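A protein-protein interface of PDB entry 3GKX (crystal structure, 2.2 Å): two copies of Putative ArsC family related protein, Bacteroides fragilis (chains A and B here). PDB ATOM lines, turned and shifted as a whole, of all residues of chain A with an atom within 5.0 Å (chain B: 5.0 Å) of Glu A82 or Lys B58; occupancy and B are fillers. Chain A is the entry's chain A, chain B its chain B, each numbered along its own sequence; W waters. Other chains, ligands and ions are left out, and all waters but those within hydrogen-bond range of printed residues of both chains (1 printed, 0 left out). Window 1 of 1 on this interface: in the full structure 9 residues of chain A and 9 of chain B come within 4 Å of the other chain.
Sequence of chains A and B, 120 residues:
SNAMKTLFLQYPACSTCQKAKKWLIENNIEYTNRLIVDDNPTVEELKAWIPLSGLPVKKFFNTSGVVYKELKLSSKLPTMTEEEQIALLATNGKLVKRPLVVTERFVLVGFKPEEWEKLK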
ATOM      1  N   VAL A  57     -23.034  -0.273  22.224  1.00  0.00           N
ATOM      2  CA  VAL A  57     -21.921  -1.119  22.615  1.00  0.00           C
ATOM      3  C   VAL A  57     -22.406  -2.427  23.235  1.00  0.00           C
ATOM      4  O   VAL A  57     -21.807  -3.514  23.051  1.00  0.00           O
ATOM      5  CB  VAL A  57     -20.970  -0.447  23.647  1.00  0.00           C
ATOM      6  CG1 VAL A  57     -19.855  -1.490  24.034  1.00  0.00           C
ATOM      7  CG2 VAL A  57     -20.348   0.830  23.093  1.00  0.00           C
ATOM      8  N   MET A  80     -22.889   0.651  33.384  1.00  0.00           N
ATOM      9  CA  MET A  80     -21.499   0.800  32.953  1.00  0.00           C
ATOM     10  C   MET A  80     -21.449   1.768  31.802  1.00  0.00           C
ATOM     11  O   MET A  80     -22.350   1.752  30.955  1.00  0.00           O
ATOM     12  CB  MET A  80     -20.954  -0.539  32.451  1.00  0.00           C
ATOM     13  CG  MET A  80     -20.984  -1.635  33.491  1.00  0.00           C
ATOM     14  SD  MET A  80     -20.317  -3.324  32.788  1.00  0.00           S
ATOM     15  CE  MET A  80     -18.519  -2.811  32.222  1.00  0.00           C
ATOM     16  N   THR A  81     -20.397   2.593  31.766  1.00  0.00           N
ATOM     17  CA  THR A  81     -20.197   3.533  30.655  1.00  0.00           C
ATOM     18  C   THR A  81     -19.751   2.750  29.415  1.00  0.00           C
ATOM     19  O   THR A  81     -19.324   1.596  29.537  1.00  0.00           O
ATOM     20  CB  THR A  81     -19.134   4.612  30.989  1.00  0.00           C
ATOM     21  OG1 THR A  81     -17.846   3.978  31.104  1.00  0.00           O
ATOM     22  CG2 THR A  81     -19.479   5.363  32.330  1.00  0.00           C
ATOM     23  N   GLU A  82     -19.856   3.374  28.241  1.00  0.00           N
ATOM     24  CA  GLU A  82     -19.354   2.782  26.987  1.00  0.00           C
ATOM     25  C   GLU A  82     -17.907   2.301  27.093  1.00  0.00           C
ATOM     26  O   GLU A  82     -17.596   1.172  26.698  1.00  0.00           O
ATOM     27  CB  GLU A  82     -19.514   3.742  25.799  1.00  0.00           C
ATOM     28  CG  GLU A  82     -20.823   3.542  25.120  1.00  0.00           C
ATOM     29  CD  GLU A  82     -21.062   4.476  23.930  1.00  0.00           C
ATOM     30  OE1 GLU A  82     -20.161   5.315  23.624  1.00  0.00           O
ATOM     31  OE2 GLU A  82     -22.171   4.357  23.307  1.00  0.00           O
ATOM     32  N   GLU A  83     -17.047   3.151  27.642  1.00  0.00           N
ATOM     33  CA  GLU A  83     -15.630   2.851  27.818  1.00  0.00           C
ATOM     34  C   GLU A  83     -15.360   1.633  28.698  1.00  0.00           C
ATOM     35  O   GLU A  83     -14.475   0.815  28.404  1.00  0.00           O
ATOM     36  CB  GLU A  83     -14.907   4.077  28.408  1.00  0.00           C
ATOM     37  CG  GLU A  83     -13.423   4.098  28.066  1.00  0.00           C
ATOM     38  CD  GLU A  83     -12.844   5.501  28.031  1.00  0.00           C
ATOM     39  OE1 GLU A  83     -13.616   6.475  27.863  1.00  0.00           O
ATOM     40  OE2 GLU A  83     -11.607   5.640  28.178  1.00  0.00           O
ATOM     41  N   GLU A  84     -16.095   1.533  29.798  1.00  0.00           N
ATOM     42  CA  GLU A  84     -16.018   0.371  30.658  1.00  0.00           C
ATOM     43  C   GLU A  84     -16.476  -0.868  29.902  1.00  0.00           C
ATOM     44  O   GLU A  84     -15.887  -1.938  30.057  1.00  0.00           O
ATOM     45  CB  GLU A  84     -16.842   0.579  31.933  1.00  0.00           C
ATOM     46  CG  GLU A  84     -16.272   1.711  32.786  1.00  0.00           C
ATOM     47  CD  GLU A  84     -17.202   2.191  33.885  1.00  0.00           C
ATOM     48  OE1 GLU A  84     -18.430   1.933  33.824  1.00  0.00           O
ATOM     49  OE2 GLU A  84     -16.683   2.846  34.821  1.00  0.00           O
ATOM     50  N   GLN A  85     -17.520  -0.735  29.088  1.00  0.00           N
ATOM     51  CA  GLN A  85     -18.056  -1.898  28.328  1.00  0.00           C
ATOM     52  C   GLN A  85     -17.013  -2.395  27.312  1.00  0.00           C
ATOM     53  O   GLN A  85     -16.755  -3.592  27.182  1.00  0.00           O
ATOM     54  CB  GLN A  85     -19.409  -1.538  27.667  1.00  0.00           C
ATOM     55  CG  GLN A  85     -20.614  -1.492  28.626  1.00  0.00           C
ATOM     56  CD  GLN A  85     -21.866  -0.793  28.021  1.00  0.00           C
ATOM     57  OE1 GLN A  85     -21.821  -0.340  26.915  1.00  0.00           O
ATOM     58  NE2 GLN A  85     -22.962  -0.704  28.774  1.00  0.00           N
ATOM     59  N   ILE A  86     -16.370  -1.453  26.635  1.00  0.00           N
ATOM     60  CA  ILE A  86     -15.344  -1.756  25.604  1.00  0.00           C
ATOM     61  C   ILE A  86     -14.092  -2.391  26.184  1.00  0.00           C
ATOM     62  O   ILE A  86     -13.531  -3.303  25.573  1.00  0.00           O
ATOM     63  CB  ILE A  86     -14.999  -0.489  24.758  1.00  0.00           C
ATOM     64  CG1 ILE A  86     -16.215  -0.135  23.871  1.00  0.00           C
ATOM     65  CG2 ILE A  86     -13.639  -0.693  23.973  1.00  0.00           C
ATOM     66  CD1 ILE A  86     -16.150   1.247  23.103  1.00  0.00           C
ATOM     67  N   PRO B  56     -28.190   3.334  19.739  1.00  0.00           N
ATOM     68  CA  PRO B  56     -27.573   3.803  20.965  1.00  0.00           C
ATOM     69  C   PRO B  56     -28.393   4.895  21.658  1.00  0.00           C
ATOM     70  O   PRO B  56     -29.106   5.685  21.020  1.00  0.00           O
ATOM     71  CB  PRO B  56     -26.191   4.358  20.491  1.00  0.00           C
ATOM     72  CG  PRO B  56     -25.920   3.671  19.201  1.00  0.00           C
ATOM     73  CD  PRO B  56     -27.284   3.501  18.581  1.00  0.00           C
ATOM     74  N   VAL B  57     -28.298   4.937  22.970  1.00  0.00           N
ATOM     75  CA  VAL B  57     -29.130   5.836  23.706  1.00  0.00           C
ATOM     76  C   VAL B  57     -28.753   7.260  23.395  1.00  0.00           C
ATOM     77  O   VAL B  57     -29.630   8.128  23.410  1.00  0.00           O
ATOM     78  CB  VAL B  57     -29.045   5.596  25.204  1.00  0.00           C
ATOM     79  CG1 VAL B  57     -29.917   6.648  25.956  1.00  0.00           C
ATOM     80  CG2 VAL B  57     -29.513   4.163  25.498  1.00  0.00           C
ATOM     81  N   LYS B  58     -27.473   7.508  23.088  1.00  0.00           N
ATOM     82  CA  LYS B  58     -27.077   8.870  22.664  1.00  0.00           C
ATOM     83  C   LYS B  58     -27.813   9.383  21.420  1.00  0.00           C
ATOM     84  O   LYS B  58     -27.994  10.588  21.286  1.00  0.00           O
ATOM     85  CB  LYS B  58     -25.555   9.023  22.551  1.00  0.00           C
ATOM     86  CG  LYS B  58     -24.883   7.994  21.705  1.00  0.00           C
ATOM     87  CD  LYS B  58     -23.393   8.204  21.764  1.00  0.00           C
ATOM     88  CE  LYS B  58     -22.669   7.235  20.853  1.00  0.00           C
ATOM     89  NZ  LYS B  58     -23.115   5.861  21.045  1.00  0.00           N
ATOM     90  N   LYS B  59     -28.281   8.472  20.552  1.00  0.00           N
ATOM     91  CA  LYS B  59     -29.012   8.851  19.331  1.00  0.00           C
ATOM     92  C   LYS B  59     -30.389   9.433  19.625  1.00  0.00           C
ATOM     93  O   LYS B  59     -31.058   9.956  18.733  1.00  0.00           O
ATOM     94  CB  LYS B  59     -29.171   7.674  18.359  1.00  0.00           C
ATOM     95  CG  LYS B  59     -27.885   7.106  17.724  1.00  0.00           C
ATOM     96  CD  LYS B  59     -27.103   8.173  17.033  1.00  0.00           C
ATOM     97  CE  LYS B  59     -26.664   7.750  15.652  1.00  0.00           C
ATOM     98  NZ  LYS B  59     -26.200   8.995  14.915  1.00  0.00           N
ATOM     99  N   PHE B  60     -30.822   9.325  20.868  1.00  0.00           N
ATOM    100  CA  PHE B  60     -32.102   9.911  21.279  1.00  0.00           C
ATOM    101  C   PHE B  60     -31.926  11.317  21.804  1.00  0.00           C
ATOM    102  O   PHE B  60     -32.873  11.895  22.339  1.00  0.00           O
ATOM    103  CB  PHE B  60     -32.767   9.051  22.345  1.00  0.00           C
ATOM    104  CG  PHE B  60     -33.526   7.882  21.773  1.00  0.00           C
ATOM    105  CD1 PHE B  60     -34.932   7.858  21.808  1.00  0.00           C
ATOM    106  CD2 PHE B  60     -32.838   6.814  21.164  1.00  0.00           C
ATOM    107  CE1 PHE B  60     -35.649   6.764  21.263  1.00  0.00           C
ATOM    108  CE2 PHE B  60     -33.542   5.752  20.629  1.00  0.00           C
ATOM    109  CZ  PHE B  60     -34.952   5.727  20.684  1.00  0.00           C
ATOM    110  N   PHE B  61     -30.713  11.865  21.672  1.00  0.00           N
ATOM    111  CA  PHE B  61     -30.481  13.236  22.066  1.00  0.00           C
ATOM    112  C   PHE B  61     -30.640  14.219  20.911  1.00  0.00           C
ATOM    113  O   PHE B  61     -30.184  13.990  19.798  1.00  0.00           O
ATOM    114  CB  PHE B  61     -29.145  13.402  22.830  1.00  0.00           C
ATOM    115  CG  PHE B  61     -29.228  12.962  24.283  1.00  0.00           C
ATOM    116  CD1 PHE B  61     -29.520  13.882  25.288  1.00  0.00           C
ATOM    117  CD2 PHE B  61     -29.073  11.615  24.638  1.00  0.00           C
ATOM    118  CE1 PHE B  61     -29.616  13.467  26.632  1.00  0.00           C
ATOM    119  CE2 PHE B  61     -29.166  11.190  25.974  1.00  0.00           C
ATOM    120  CZ  PHE B  61     -29.441  12.115  26.965  1.00  0.00           C
ATOM    121  N   LEU B  77     -21.926  12.953  27.994  1.00  0.00           N
ATOM    122  CA  LEU B  77     -22.741  11.767  27.736  1.00  0.00           C
ATOM    123  C   LEU B  77     -21.988  10.464  27.899  1.00  0.00           C
ATOM    124  O   LEU B  77     -22.554   9.510  28.449  1.00  0.00           O
ATOM    125  CB  LEU B  77     -23.418  11.778  26.350  1.00  0.00           C
ATOM    126  CG  LEU B  77     -24.717  12.542  26.043  1.00  0.00           C
ATOM    127  CD1 LEU B  77     -25.116  12.230  24.618  1.00  0.00           C
ATOM    128  CD2 LEU B  77     -25.871  12.221  26.987  1.00  0.00           C
ATOM    129  N   PRO B  78     -20.738  10.395  27.380  1.00  0.00           N
ATOM    130  CA  PRO B  78     -20.026   9.144  27.542  1.00  0.00           C
ATOM    131  C   PRO B  78     -20.022   8.700  29.001  1.00  0.00           C
ATOM    132  O   PRO B  78     -20.707   7.717  29.341  1.00  0.00           O
ATOM    133  CB  PRO B  78     -18.633   9.481  27.028  1.00  0.00           C
ATOM    134  CG  PRO B  78     -18.931  10.377  25.887  1.00  0.00           C
ATOM    135  CD  PRO B  78     -20.088  11.238  26.359  1.00  0.00           C
ATOM    136  N   GLN B  85     -28.285   8.326  31.439  1.00  0.00           N
ATOM    137  CA  GLN B  85     -28.754   8.923  30.183  1.00  0.00           C
ATOM    138  C   GLN B  85     -30.287   8.865  30.018  1.00  0.00           C
ATOM    139  O   GLN B  85     -30.893   9.844  29.621  1.00  0.00           O
ATOM    140  CB  GLN B  85     -28.091   8.246  28.984  1.00  0.00           C
ATOM    141  CG  GLN B  85     -26.642   8.649  28.743  1.00  0.00           C
ATOM    142  CD  GLN B  85     -25.940   7.683  27.832  1.00  0.00           C
ATOM    143  OE1 GLN B  85     -26.564   6.789  27.279  1.00  0.00           O
ATOM    144  NE2 GLN B  85     -24.630   7.842  27.676  1.00  0.00           N
HETATM  145  O   HOH W   1     -21.365   5.653  27.909  1.00  0.00           O
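The side-chain carboxylate (OE2) of Glu A82 is in salt-bridge range of the side-chain amino group (NZ) of Lys B58, at 2.9 Å.
The side-chain carboxylate of Glu A84 is in hydrogen-bond range of the backbone NH of Thr A81 (2.9 Å).
Thr A81 touches Pro B78 (CB to O, 3.9 Å).
Printed residues of chain B within 4 Å of Thr A81: Pro B78. Of the printed residues of chain B, Glu A82 touches Lys B58. Val B57 touches none of the printed residues of chain A. Lys B58 touches just one residue of chain A: Glu A82. Phe B61 touches none of the printed residues of chain A. Of the printed residues of chain A, Pro B78 touches Thr A81 (3.9 Å). The nearest printed residue of chain A that does not touch Lys B58 is Val A57 (6.1 Å). The nearest printed residue of chain A that does not touch Pro B78 is Glu A82 (4.6 Å).
Printed residues of chain B that touch a printed residue of chain A: Lys B58 and Pro B78. Along chain B the printed residues that touch a printed residue of chain A span positions 58 to 78. Among the printed residues, 2 pairs touch across the chains. Among the printed residues, Asp or Glu carboxylates within 4 Å of a Lys or Arg side-chain nitrogen of the other chain: Glu A82 with Lys B58 (2.9 Å).
2 positions are printed for both chains. Of the 2 pairs that touch across the chains among the printed residues, none has its exchanged pair printed and touching as well.
Water W1 bridges O of Pro B78 (2.6 Å) and N of Glu A82 (2.8 Å).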
